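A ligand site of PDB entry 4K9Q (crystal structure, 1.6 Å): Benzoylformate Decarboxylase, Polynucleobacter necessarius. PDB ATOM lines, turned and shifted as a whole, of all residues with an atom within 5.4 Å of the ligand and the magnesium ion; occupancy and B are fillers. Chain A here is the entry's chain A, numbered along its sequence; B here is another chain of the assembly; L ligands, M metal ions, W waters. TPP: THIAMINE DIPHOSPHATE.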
ATOM      1  N   TYR A 278      41.893   0.812  -8.189  1.00  0.00           N
ATOM      2  CA  TYR A 278      40.856   1.830  -8.030  1.00  0.00           C
ATOM      3  C   TYR A 278      41.468   3.190  -7.658  1.00  0.00           C
ATOM      4  O   TYR A 278      41.574   4.067  -8.506  1.00  0.00           O
ATOM      5  CB  TYR A 278      39.776   1.367  -7.041  1.00  0.00           C
ATOM      6  CG  TYR A 278      38.638   2.345  -6.850  1.00  0.00           C
ATOM      7  CD1 TYR A 278      38.358   3.321  -7.798  1.00  0.00           C
ATOM      8  CD2 TYR A 278      37.842   2.281  -5.718  1.00  0.00           C
ATOM      9  CE1 TYR A 278      37.324   4.226  -7.611  1.00  0.00           C
ATOM     10  CE2 TYR A 278      36.793   3.161  -5.528  1.00  0.00           C
ATOM     11  CZ  TYR A 278      36.543   4.135  -6.481  1.00  0.00           C
ATOM     12  OH  TYR A 278      35.491   5.023  -6.293  1.00  0.00           O
ATOM     13  N   GLU A 372      26.757  -4.280  -1.083  1.00  0.00           N
ATOM     14  CA  GLU A 372      26.950  -2.984  -1.733  1.00  0.00           C
ATOM     15  C   GLU A 372      26.887  -1.932  -0.643  1.00  0.00           C
ATOM     16  O   GLU A 372      25.933  -1.169  -0.533  1.00  0.00           O
ATOM     17  CB  GLU A 372      25.879  -2.739  -2.801  1.00  0.00           C
ATOM     18  CG  GLU A 372      26.163  -1.539  -3.710  1.00  0.00           C
ATOM     19  CD  GLU A 372      25.168  -1.413  -4.847  1.00  0.00           C
ATOM     20  OE1 GLU A 372      25.175  -2.258  -5.765  1.00  0.00           O
ATOM     21  OE2 GLU A 372      24.354  -0.464  -4.807  1.00  0.00           O
ATOM     22  N   CYS A 373      27.924  -1.940   0.199  1.00  0.00           N
ATOM     23  CA  CYS A 373      28.058  -0.997   1.308  1.00  0.00           C
ATOM     24  C   CYS A 373      29.539  -0.693   1.348  1.00  0.00           C
ATOM     25  O   CYS A 373      30.293  -1.303   2.110  1.00  0.00           O
ATOM     26  CB  CYS A 373      27.598  -1.650   2.614  1.00  0.00           C
ATOM     27  SG  CYS A 373      27.441  -0.470   3.961  1.00  0.00           S
ATOM     28  N   PRO A 374      29.979   0.238   0.494  1.00  0.00           N
ATOM     29  CA  PRO A 374      31.413   0.373   0.225  1.00  0.00           C
ATOM     30  C   PRO A 374      32.304   0.579   1.443  1.00  0.00           C
ATOM     31  O   PRO A 374      33.362  -0.066   1.524  1.00  0.00           O
ATOM     32  CB  PRO A 374      31.463   1.591  -0.711  1.00  0.00           C
ATOM     33  CG  PRO A 374      30.171   1.491  -1.485  1.00  0.00           C
ATOM     34  CD  PRO A 374      29.154   1.033  -0.434  1.00  0.00           C
ATOM     35  N   SER A 375      31.910   1.423   2.392  1.00  0.00           N
ATOM     36  CA  SER A 375      32.830   1.732   3.496  1.00  0.00           C
ATOM     37  C   SER A 375      33.118   0.545   4.418  1.00  0.00           C
ATOM     38  O   SER A 375      34.140   0.536   5.097  1.00  0.00           O
ATOM     39  CB  SER A 375      32.341   2.936   4.319  1.00  0.00           C
ATOM     40  OG  SER A 375      31.222   2.594   5.104  1.00  0.00           O
ATOM     41  N   ILE A 376      32.250  -0.473   4.432  1.00  0.00           N
ATOM     42  CA  ILE A 376      32.435  -1.600   5.348  1.00  0.00           C
ATOM     43  C   ILE A 376      33.103  -2.839   4.742  1.00  0.00           C
ATOM     44  O   ILE A 376      33.277  -3.855   5.414  1.00  0.00           O
ATOM     45  CB  ILE A 376      31.103  -2.042   6.040  1.00  0.00           C
ATOM     46  CG1 ILE A 376      30.177  -2.732   5.035  1.00  0.00           C
ATOM     47  CG2 ILE A 376      30.426  -0.848   6.699  1.00  0.00           C
ATOM     48  CD1 ILE A 376      28.911  -3.315   5.675  1.00  0.00           C
ATOM     49  N   GLY A 398      31.661  -1.634  -9.821  1.00  0.00           N
ATOM     50  CA  GLY A 398      31.551  -0.510  -8.903  1.00  0.00           C
ATOM     51  C   GLY A 398      30.345   0.396  -9.129  1.00  0.00           C
ATOM     52  O   GLY A 398      30.211   1.421  -8.446  1.00  0.00           O
ATOM     53  N   GLY A 399      29.475   0.047 -10.071  1.00  0.00           N
ATOM     54  CA  GLY A 399      28.286   0.836 -10.354  1.00  0.00           C
ATOM     55  C   GLY A 399      27.143   0.610  -9.374  1.00  0.00           C
ATOM     56  O   GLY A 399      26.468  -0.419  -9.417  1.00  0.00           O
ATOM     57  N   LEU A 400      26.922   1.575  -8.498  1.00  0.00           N
ATOM     58  CA  LEU A 400      25.880   1.445  -7.493  1.00  0.00           C
ATOM     59  C   LEU A 400      24.498   1.313  -8.133  1.00  0.00           C
ATOM     60  O   LEU A 400      24.246   1.850  -9.219  1.00  0.00           O
ATOM     61  CB  LEU A 400      25.901   2.647  -6.542  1.00  0.00           C
ATOM     62  CG  LEU A 400      27.215   2.858  -5.792  1.00  0.00           C
ATOM     63  CD1 LEU A 400      27.086   4.068  -4.852  1.00  0.00           C
ATOM     64  CD2 LEU A 400      27.570   1.597  -5.003  1.00  0.00           C
ATOM     65  N   GLY A 428      24.612  -0.089   1.849  1.00  0.00           N
ATOM     66  CA  GLY A 428      24.769   1.248   2.399  1.00  0.00           C
ATOM     67  C   GLY A 428      23.488   2.046   2.200  1.00  0.00           C
ATOM     68  O   GLY A 428      22.688   1.733   1.300  1.00  0.00           O
ATOM     69  N   ASP A 429      23.275   3.074   3.010  1.00  0.00           N
ATOM     70  CA  ASP A 429      22.081   3.903   2.852  1.00  0.00           C
ATOM     71  C   ASP A 429      22.057   4.703   1.525  1.00  0.00           C
ATOM     72  O   ASP A 429      21.005   4.861   0.918  1.00  0.00           O
ATOM     73  CB  ASP A 429      21.779   4.783   4.080  1.00  0.00           C
ATOM     74  CG  ASP A 429      22.945   5.659   4.512  1.00  0.00           C
ATOM     75  OD1 ASP A 429      24.081   5.409   4.092  1.00  0.00           O
ATOM     76  OD2 ASP A 429      22.720   6.594   5.317  1.00  0.00           O
ATOM     77  N   GLY A 430      23.227   5.195   1.098  1.00  0.00           N
ATOM     78  CA  GLY A 430      23.340   5.844  -0.200  1.00  0.00           C
ATOM     79  C   GLY A 430      23.102   4.876  -1.349  1.00  0.00           C
ATOM     80  O   GLY A 430      22.307   5.141  -2.258  1.00  0.00           O
ATOM     81  N   SER A 431      23.809   3.744  -1.309  1.00  0.00           N
ATOM     82  CA  SER A 431      23.684   2.715  -2.340  1.00  0.00           C
ATOM     83  C   SER A 431      22.251   2.235  -2.499  1.00  0.00           C
ATOM     84  O   SER A 431      21.794   2.004  -3.612  1.00  0.00           O
ATOM     85  CB  SER A 431      24.582   1.506  -2.005  1.00  0.00           C
ATOM     86  OG  SER A 431      25.952   1.823  -2.152  1.00  0.00           O
ATOM     87  N   PHE A 432      21.558   2.076  -1.372  1.00  0.00           N
ATOM     88  CA  PHE A 432      20.173   1.596  -1.336  1.00  0.00           C
ATOM     89  C   PHE A 432      19.240   2.410  -2.249  1.00  0.00           C
ATOM     90  O   PHE A 432      18.291   1.863  -2.813  1.00  0.00           O
ATOM     91  CB  PHE A 432      19.672   1.674   0.116  1.00  0.00           C
ATOM     92  CG  PHE A 432      18.427   0.860   0.411  1.00  0.00           C
ATOM     93  CD1 PHE A 432      18.503  -0.516   0.559  1.00  0.00           C
ATOM     94  CD2 PHE A 432      17.218   1.488   0.613  1.00  0.00           C
ATOM     95  CE1 PHE A 432      17.363  -1.255   0.870  1.00  0.00           C
ATOM     96  CE2 PHE A 432      16.077   0.763   0.935  1.00  0.00           C
ATOM     97  CZ  PHE A 432      16.158  -0.609   1.051  1.00  0.00           C
ATOM     98  N   TYR A 434      19.754   3.957  -5.235  1.00  0.00           N
ATOM     99  CA  TYR A 434      19.875   4.003  -6.691  1.00  0.00           C
ATOM    100  C   TYR A 434      18.814   3.173  -7.400  1.00  0.00           C
ATOM    101  O   TYR A 434      18.220   3.625  -8.377  1.00  0.00           O
ATOM    102  CB  TYR A 434      21.273   3.583  -7.169  1.00  0.00           C
ATOM    103  CG  TYR A 434      22.332   4.619  -6.819  1.00  0.00           C
ATOM    104  CD1 TYR A 434      22.902   4.667  -5.549  1.00  0.00           C
ATOM    105  CD2 TYR A 434      22.777   5.537  -7.775  1.00  0.00           C
ATOM    106  CE1 TYR A 434      23.849   5.610  -5.232  1.00  0.00           C
ATOM    107  CE2 TYR A 434      23.736   6.484  -7.461  1.00  0.00           C
ATOM    108  CZ  TYR A 434      24.272   6.521  -6.189  1.00  0.00           C
ATOM    109  OH  TYR A 434      25.221   7.442  -5.834  1.00  0.00           O
ATOM    110  N   PHE A 454      23.022  -0.288   6.397  1.00  0.00           N
ATOM    111  CA  PHE A 454      23.943   0.377   7.306  1.00  0.00           C
ATOM    112  C   PHE A 454      23.802   1.886   7.173  1.00  0.00           C
ATOM    113  O   PHE A 454      24.313   2.496   6.241  1.00  0.00           O
ATOM    114  CB  PHE A 454      25.380  -0.070   7.017  1.00  0.00           C
ATOM    115  CG  PHE A 454      25.643  -1.513   7.377  1.00  0.00           C
ATOM    116  CD1 PHE A 454      25.064  -2.543   6.653  1.00  0.00           C
ATOM    117  CD2 PHE A 454      26.454  -1.829   8.450  1.00  0.00           C
ATOM    118  CE1 PHE A 454      25.297  -3.868   7.003  1.00  0.00           C
ATOM    119  CE2 PHE A 454      26.700  -3.150   8.797  1.00  0.00           C
ATOM    120  CZ  PHE A 454      26.121  -4.181   8.073  1.00  0.00           C
ATOM    121  N   ASN A 456      24.653   5.410   7.962  1.00  0.00           N
ATOM    122  CA  ASN A 456      25.543   6.434   8.515  1.00  0.00           C
ATOM    123  C   ASN A 456      25.206   7.851   8.027  1.00  0.00           C
ATOM    124  O   ASN A 456      25.913   8.813   8.326  1.00  0.00           O
ATOM    125  CB  ASN A 456      27.030   6.105   8.277  1.00  0.00           C
ATOM    126  CG  ASN A 456      27.359   5.876   6.816  1.00  0.00           C
ATOM    127  OD1 ASN A 456      26.545   6.145   5.953  1.00  0.00           O
ATOM    128  ND2 ASN A 456      28.566   5.379   6.527  1.00  0.00           N
ATOM    129  N   GLU A 457      24.088   7.970   7.309  1.00  0.00           N
ATOM    130  CA  GLU A 457      23.596   9.244   6.776  1.00  0.00           C
ATOM    131  C   GLU A 457      24.622   9.986   5.936  1.00  0.00           C
ATOM    132  O   GLU A 457      24.672  11.219   5.952  1.00  0.00           O
ATOM    133  CB  GLU A 457      23.076  10.132   7.916  1.00  0.00           C
ATOM    134  CG  GLU A 457      22.019   9.415   8.725  1.00  0.00           C
ATOM    135  CD  GLU A 457      21.228  10.325   9.639  1.00  0.00           C
ATOM    136  OE1 GLU A 457      21.851  11.034  10.456  1.00  0.00           O
ATOM    137  OE2 GLU A 457      19.981  10.341   9.537  1.00  0.00           O
ATOM    138  N   GLU A 458      25.427   9.243   5.192  1.00  0.00           N
ATOM    139  CA  GLU A 458      26.462   9.845   4.349  1.00  0.00           C
ATOM    140  C   GLU A 458      26.920   8.901   3.254  1.00  0.00           C
ATOM    141  O   GLU A 458      26.692   7.694   3.340  1.00  0.00           O
ATOM    142  CB  GLU A 458      27.674  10.235   5.220  1.00  0.00           C
ATOM    143  CG  GLU A 458      28.415   9.019   5.800  1.00  0.00           C
ATOM    144  CD  GLU A 458      29.376   9.365   6.952  1.00  0.00           C
ATOM    145  OE1 GLU A 458      29.630  10.562   7.188  1.00  0.00           O
ATOM    146  OE2 GLU A 458      29.862   8.413   7.603  1.00  0.00           O
ATOM    147  N   TYR A 459      27.555   9.434   2.223  1.00  0.00           N
ATOM    148  CA  TYR A 459      28.288   8.616   1.284  1.00  0.00           C
ATOM    149  C   TYR A 459      29.678   8.408   1.902  1.00  0.00           C
ATOM    150  O   TYR A 459      30.641   9.098   1.565  1.00  0.00           O
ATOM    151  CB  TYR A 459      28.406   9.333  -0.059  1.00  0.00           C
ATOM    152  CG  TYR A 459      27.140   9.430  -0.915  1.00  0.00           C
ATOM    153  CD1 TYR A 459      26.302   8.327  -1.151  1.00  0.00           C
ATOM    154  CD2 TYR A 459      26.810  10.629  -1.546  1.00  0.00           C
ATOM    155  CE1 TYR A 459      25.176   8.430  -1.967  1.00  0.00           C
ATOM    156  CE2 TYR A 459      25.692  10.735  -2.358  1.00  0.00           C
ATOM    157  CZ  TYR A 459      24.888   9.639  -2.572  1.00  0.00           C
ATOM    158  OH  TYR A 459      23.776   9.768  -3.393  1.00  0.00           O
ATOM    159  N   GLY A 460      29.764   7.474   2.858  1.00  0.00           N
ATOM    160  CA  GLY A 460      30.939   7.329   3.695  1.00  0.00           C
ATOM    161  C   GLY A 460      32.248   7.158   2.944  1.00  0.00           C
ATOM    162  O   GLY A 460      33.247   7.822   3.242  1.00  0.00           O
ATOM    163  N   ILE A 461      32.249   6.256   1.977  1.00  0.00           N
ATOM    164  CA  ILE A 461      33.503   5.953   1.301  1.00  0.00           C
ATOM    165  C   ILE A 461      34.001   7.158   0.500  1.00  0.00           C
ATOM    166  O   ILE A 461      35.200   7.301   0.298  1.00  0.00           O
ATOM    167  CB  ILE A 461      33.414   4.692   0.427  1.00  0.00           C
ATOM    168  CG1 ILE A 461      34.833   4.224   0.081  1.00  0.00           C
ATOM    169  CG2 ILE A 461      32.612   4.969  -0.817  1.00  0.00           C
ATOM    170  CD1 ILE A 461      34.905   2.875  -0.585  1.00  0.00           C
ATOM    171  N   LEU A 462      33.089   8.033   0.069  1.00  0.00           N
ATOM    172  CA  LEU A 462      33.547   9.252  -0.615  1.00  0.00           C
ATOM    173  C   LEU A 462      34.284  10.199   0.338  1.00  0.00           C
ATOM    174  O   LEU A 462      35.164  10.958  -0.088  1.00  0.00           O
ATOM    175  CB  LEU A 462      32.403   9.976  -1.316  1.00  0.00           C
ATOM    176  CG  LEU A 462      31.688   9.195  -2.424  1.00  0.00           C
ATOM    177  CD1 LEU A 462      30.660  10.070  -3.126  1.00  0.00           C
ATOM    178  CD2 LEU A 462      32.684   8.601  -3.417  1.00  0.00           C
ATOM    179  N   LEU A 479      23.770  12.673   3.737  1.00  0.00           N
ATOM    180  CA  LEU A 479      22.439  12.185   3.395  1.00  0.00           C
ATOM    181  C   LEU A 479      21.444  12.267   4.565  1.00  0.00           C
ATOM    182  O   LEU A 479      20.900  11.248   4.993  1.00  0.00           O
ATOM    183  CB  LEU A 479      22.515  10.735   2.933  1.00  0.00           C
ATOM    184  CG  LEU A 479      23.381  10.442   1.712  1.00  0.00           C
ATOM    185  CD1 LEU A 479      23.488   8.935   1.458  1.00  0.00           C
ATOM    186  CD2 LEU A 479      22.843  11.189   0.479  1.00  0.00           C
ATOM    187  N   LEU A 528      34.538   7.004  10.187  1.00  0.00           N
ATOM    188  CA  LEU A 528      34.976   6.123   9.114  1.00  0.00           C
ATOM    189  C   LEU A 528      36.433   5.742   9.283  1.00  0.00           C
ATOM    190  O   LEU A 528      37.284   6.588   9.567  1.00  0.00           O
ATOM    191  CB  LEU A 528      34.785   6.812   7.757  1.00  0.00           C
ATOM    192  CG  LEU A 528      33.349   7.146   7.319  1.00  0.00           C
ATOM    193  CD1 LEU A 528      33.357   8.304   6.334  1.00  0.00           C
ATOM    194  CD2 LEU A 528      32.680   5.909   6.686  1.00  0.00           C
ATOM    195  N   ASN B  23      25.563  13.819  -8.894  1.00  0.00           N
ATOM    196  CA  ASN B  23      25.663  12.754  -7.914  1.00  0.00           C
ATOM    197  C   ASN B  23      27.134  12.382  -7.901  1.00  0.00           C
ATOM    198  O   ASN B  23      27.678  11.943  -8.931  1.00  0.00           O
ATOM    199  CB  ASN B  23      24.774  11.575  -8.297  1.00  0.00           C
ATOM    200  CG  ASN B  23      24.900  10.419  -7.323  1.00  0.00           C
ATOM    201  OD1 ASN B  23      25.645   9.463  -7.558  1.00  0.00           O
ATOM    202  ND2 ASN B  23      24.172  10.495  -6.210  1.00  0.00           N
ATOM    203  N   PRO B  24      27.819  12.614  -6.764  1.00  0.00           N
ATOM    204  CA  PRO B  24      29.282  12.574  -6.764  1.00  0.00           C
ATOM    205  C   PRO B  24      29.878  11.162  -6.728  1.00  0.00           C
ATOM    206  O   PRO B  24      29.214  10.212  -6.330  1.00  0.00           O
ATOM    207  CB  PRO B  24      29.636  13.337  -5.467  1.00  0.00           C
ATOM    208  CG  PRO B  24      28.488  13.058  -4.561  1.00  0.00           C
ATOM    209  CD  PRO B  24      27.275  13.032  -5.463  1.00  0.00           C
ATOM    210  N   GLY B  25      31.133  11.058  -7.172  1.00  0.00           N
ATOM    211  CA  GLY B  25      31.900   9.833  -7.070  1.00  0.00           C
ATOM    212  C   GLY B  25      33.367  10.212  -6.924  1.00  0.00           C
ATOM    213  O   GLY B  25      33.707  11.395  -6.963  1.00  0.00           O
ATOM    214  N   SER B  26      34.240   9.217  -6.749  1.00  0.00           N
ATOM    215  CA  SER B  26      35.646   9.487  -6.473  1.00  0.00           C
ATOM    216  C   SER B  26      36.307  10.257  -7.598  1.00  0.00           C
ATOM    217  O   SER B  26      37.164  11.116  -7.357  1.00  0.00           O
ATOM    218  CB  SER B  26      36.405   8.175  -6.221  1.00  0.00           C
ATOM    219  OG  SER B  26      36.483   7.401  -7.402  1.00  0.00           O
ATOM    220  N   GLU B  47      21.143   9.144 -11.078  1.00  0.00           N
ATOM    221  CA  GLU B  47      21.543   9.987 -12.191  1.00  0.00           C
ATOM    222  C   GLU B  47      20.448  10.349 -13.194  1.00  0.00           C
ATOM    223  O   GLU B  47      20.539  11.360 -13.877  1.00  0.00           O
ATOM    224  CB  GLU B  47      22.780   9.412 -12.883  1.00  0.00           C
ATOM    225  CG  GLU B  47      24.007   9.370 -11.969  1.00  0.00           C
ATOM    226  CD  GLU B  47      24.095   8.124 -11.087  1.00  0.00           C
ATOM    227  OE1 GLU B  47      23.121   7.343 -11.014  1.00  0.00           O
ATOM    228  OE2 GLU B  47      25.162   7.946 -10.446  1.00  0.00           O
ATOM    229  N   HIS B  70      29.165  10.275 -12.267  1.00  0.00           N
ATOM    230  CA  HIS B  70      30.321   9.451 -11.944  1.00  0.00           C
ATOM    231  C   HIS B  70      30.644   8.447 -13.040  1.00  0.00           C
ATOM    232  O   HIS B  70      30.062   7.373 -13.093  1.00  0.00           O
ATOM    233  CB  HIS B  70      30.086   8.705 -10.638  1.00  0.00           C
ATOM    234  CG  HIS B  70      31.219   7.806 -10.234  1.00  0.00           C
ATOM    235  ND1 HIS B  70      32.504   8.271 -10.050  1.00  0.00           N
ATOM    236  CD2 HIS B  70      31.255   6.484  -9.983  1.00  0.00           C
ATOM    237  CE1 HIS B  70      33.281   7.266  -9.687  1.00  0.00           C
ATOM    238  NE2 HIS B  70      32.547   6.176  -9.623  1.00  0.00           N
ATOM    239  N   ALA B  73      29.375   4.463 -14.960  1.00  0.00           N
ATOM    240  CA  ALA B  73      28.272   3.967 -14.114  1.00  0.00           C
ATOM    241  C   ALA B  73      27.171   5.011 -14.019  1.00  0.00           C
ATOM    242  O   ALA B  73      25.989   4.706 -14.191  1.00  0.00           O
ATOM    243  CB  ALA B  73      28.783   3.631 -12.720  1.00  0.00           C
ATOM    244  N   GLY B  74      27.574   6.235 -13.714  1.00  0.00           N
ATOM    245  CA  GLY B  74      26.648   7.341 -13.582  1.00  0.00           C
ATOM    246  C   GLY B  74      26.058   7.716 -14.921  1.00  0.00           C
ATOM    247  O   GLY B  74      24.845   7.936 -15.042  1.00  0.00           O
ATOM    248  N   ASN B  77      23.299   5.203 -15.855  1.00  0.00           N
ATOM    249  CA  ASN B  77      22.032   5.426 -15.174  1.00  0.00           C
ATOM    250  C   ASN B  77      21.264   6.612 -15.747  1.00  0.00           C
ATOM    251  O   ASN B  77      20.022   6.696 -15.623  1.00  0.00           O
ATOM    252  CB  ASN B  77      22.245   5.643 -13.671  1.00  0.00           C
ATOM    253  CG  ASN B  77      22.500   4.348 -12.919  1.00  0.00           C
ATOM    254  OD1 ASN B  77      22.345   3.261 -13.474  1.00  0.00           O
ATOM    255  ND2 ASN B  77      22.881   4.470 -11.651  1.00  0.00           N
ATOM    256  N   LEU B 110      36.213   1.381 -12.764  1.00  0.00           N
ATOM    257  CA  LEU B 110      35.490   2.641 -12.969  1.00  0.00           C
ATOM    258  C   LEU B 110      36.104   3.521 -14.067  1.00  0.00           C
ATOM    259  O   LEU B 110      35.882   4.738 -14.114  1.00  0.00           O
ATOM    260  CB  LEU B 110      35.274   3.381 -11.637  1.00  0.00           C
ATOM    261  CG  LEU B 110      34.225   2.671 -10.765  1.00  0.00           C
ATOM    262  CD1 LEU B 110      34.381   2.982  -9.287  1.00  0.00           C
ATOM    263  CD2 LEU B 110      32.800   2.992 -11.231  1.00  0.00           C
HETATM  264  N1' TPP L   1      26.847   6.617  -8.868  1.00  0.00           N
HETATM  265  C2' TPP L   1      26.916   5.311  -9.314  1.00  0.00           C
HETATM  266  CM2 TPP L   1      25.858   4.770 -10.227  1.00  0.00           C
HETATM  267  N3' TPP L   1      27.958   4.479  -8.944  1.00  0.00           N
HETATM  268  C4' TPP L   1      28.941   4.963  -8.111  1.00  0.00           C
HETATM  269  N4' TPP L   1      29.957   4.169  -7.771  1.00  0.00           N
HETATM  270  C5' TPP L   1      28.867   6.265  -7.633  1.00  0.00           C
HETATM  271  C6' TPP L   1      27.832   7.105  -8.022  1.00  0.00           C
HETATM  272  C7' TPP L   1      29.958   6.795  -6.722  1.00  0.00           C
HETATM  273  N3  TPP L   1      29.989   6.267  -5.363  1.00  0.00           N
HETATM  274  C2  TPP L   1      30.864   5.296  -4.917  1.00  0.00           C
HETATM  275  S1  TPP L   1      30.708   4.923  -3.359  1.00  0.00           S
HETATM  276  C5  TPP L   1      29.524   6.012  -3.186  1.00  0.00           C
HETATM  277  C4  TPP L   1      29.201   6.710  -4.354  1.00  0.00           C
HETATM  278  CM4 TPP L   1      28.139   7.768  -4.483  1.00  0.00           C
HETATM  279  C6  TPP L   1      28.946   6.153  -1.806  1.00  0.00           C
HETATM  280  C7  TPP L   1      28.273   4.911  -1.254  1.00  0.00           C
HETATM  281  O7  TPP L   1      27.593   5.342  -0.097  1.00  0.00           O
HETATM  282  PA  TPP L   1      26.807   4.313   0.863  1.00  0.00           P
HETATM  283  O1A TPP L   1      26.062   3.333   0.012  1.00  0.00           O
HETATM  284  O2A TPP L   1      25.889   5.055   1.772  1.00  0.00           O
HETATM  285  O3A TPP L   1      27.977   3.479   1.570  1.00  0.00           O
HETATM  286  PB  TPP L   1      29.002   3.965   2.711  1.00  0.00           P
HETATM  287  O1B TPP L   1      30.266   4.357   2.003  1.00  0.00           O
HETATM  288  O2B TPP L   1      29.239   2.764   3.602  1.00  0.00           O
HETATM  289  O3B TPP L   1      28.466   5.137   3.471  1.00  0.00           O
HETATM  290 MG    MG M   1      26.282   5.507   3.876  1.00  0.00          MG
HETATM  291  O   HOH W   1      26.320   3.266   4.560  1.00  0.00           O
HETATM  292  O   HOH W   2      32.611   4.553  -7.442  1.00  0.00           O
HETATM  293  O   HOH W   3      33.176   2.810  -4.219  1.00  0.00           O
HETATM  294  O   HOH W   4      32.022   2.109  -6.352  1.00  0.00           O
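The side-chain hydroxyl (OG) of Ser 431 lies within hydrogen-bond range of an oxygen (O1A) of the ligand. OG of Ser 375 is in hydrogen-bond range of O2B of the ligand (2.5 Å). N of Ile 461 lies within hydrogen-bond range of O1B of the ligand (2.7 Å). O of Gly 398 is in hydrogen-bond range of N4' of the ligand (2.8 Å). An oxygen (O2B) of the ligand sits close to the backbone NH of Ser 375. SG of Cys 373 is in hydrogen-bond range of O2B of the ligand. N3' of the ligand sits at hydrogen-bond distance from N of Leu 400, at 3.1 Å. The backbone NH (N) of Ser 431 lies within hydrogen-bond range of an oxygen (O1A) of the ligand (2.6 Å). A nitrogen (N1') of the ligand sits close to the side-chain amide oxygen of Asn 23 of chain B (3.4 Å). O2A of the ligand lies close to N of Gly 430, 2.7 Å away. O1B of the ligand lies within hydrogen-bond range of N of Gly 460 (3.3 Å). The side-chain carboxylate (OE2) of Glu 47 of chain B sits at hydrogen-bond distance from a nitrogen (N1') of the ligand (2.7 Å).
The side-chain amide oxygen (OD1) of Asn 23 of chain B sits close to the side-chain carboxylate (OE2) of Glu 47 of chain B, 3.3 Å away. The side-chain carboxylate (OD2) of Asp 429 sits at hydrogen-bond distance from the backbone NH (N) of Glu 457 (2.8 Å). The side-chain hydroxyl of Tyr 434 sits at hydrogen-bond distance from the side-chain amide oxygen of Asn 23 of chain B (2.7 Å). The backbone NH of Gly 428 lies within hydrogen-bond range of the backbone carbonyl oxygen of Glu 372, at 2.9 Å. ND2 of Asn 23 of chain B is in hydrogen-bond range of OH of Tyr 459 (2.9 Å). The side-chain sulfur (SG) of Cys 373 lies close to the backbone NH (N) of Gly 428. The side-chain carboxylate (OE1) of Glu 47 of chain B sits at hydrogen-bond distance from the side-chain amide nitrogen (ND2) of Asn 77 of chain B, 3.0 Å away. The backbone NH of Asp 429 lies within hydrogen-bond range of the backbone carbonyl oxygen of Phe 454, 3.4 Å away.
CD of Pro 374 touches O3A of the ligand (3.4 Å). Gly 399 touches the ligand. CA of Gly 428 touches O1A of the ligand (3.4 Å). OH of Tyr 434 touches CM4 of the ligand (3.2 Å). Tyr 459 touches the ligand. Leu 462 touches the ligand (CD1 to CM4, 3.7 Å). Pro 24 of chain B touches the ligand. Gly 25 of chain B touches the ligand. His 70 of chain B touches the ligand (CD2 to C4', 3.3 Å). CB of Ala 73 of chain B touches N3' of the ligand, 3.96 Å away. Asn 77 of chain B touches the ligand (ND2 to CM2, 3.3 Å). Of the 35 residues printed, 24 come within 4 Å of the ligand. Along chain A the residues within 4 Å of the ligand span positions 373 to 462. The nearest printed residue that does not touch the ligand is Gly 74 of chain B (4.2 Å).
Of the 35 residues printed, 3 come within 4 Å of the magnesium ion. The nearest printed residue that does not touch the magnesium ion is Gly 460 (4.1 Å).
O2A of the ligand binds the magnesium ion, at 2.2 Å. OD1 of Asn 456 binds the magnesium ion (2.2 Å). The magnesium ion is bound by OD1 of Asp 429, at 2.2 Å. O3B of the ligand binds the magnesium ion (2.3 Å). The magnesium ion is bound by O of Glu 458, at 2.3 Å. The magnesium ion is bound by water W1 (2.3 Å). The magnesium ion has six donor atoms within binding distance.
Water W1 lies within hydrogen-bond range of O of Phe 454 (2.7 Å), O2B of the ligand (3.1 Å) and N of Asp 429 (3.4 Å). Water W2 lies within hydrogen-bond range of a nitrogen (N4') of the ligand, a ring nitrogen (NE2) of His 70 of chain B and the side-chain hydroxyl of Tyr 278. Water W4 bridges O of Gly 398 (2.9 Å) and N4' of the ligand (3.2 Å).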
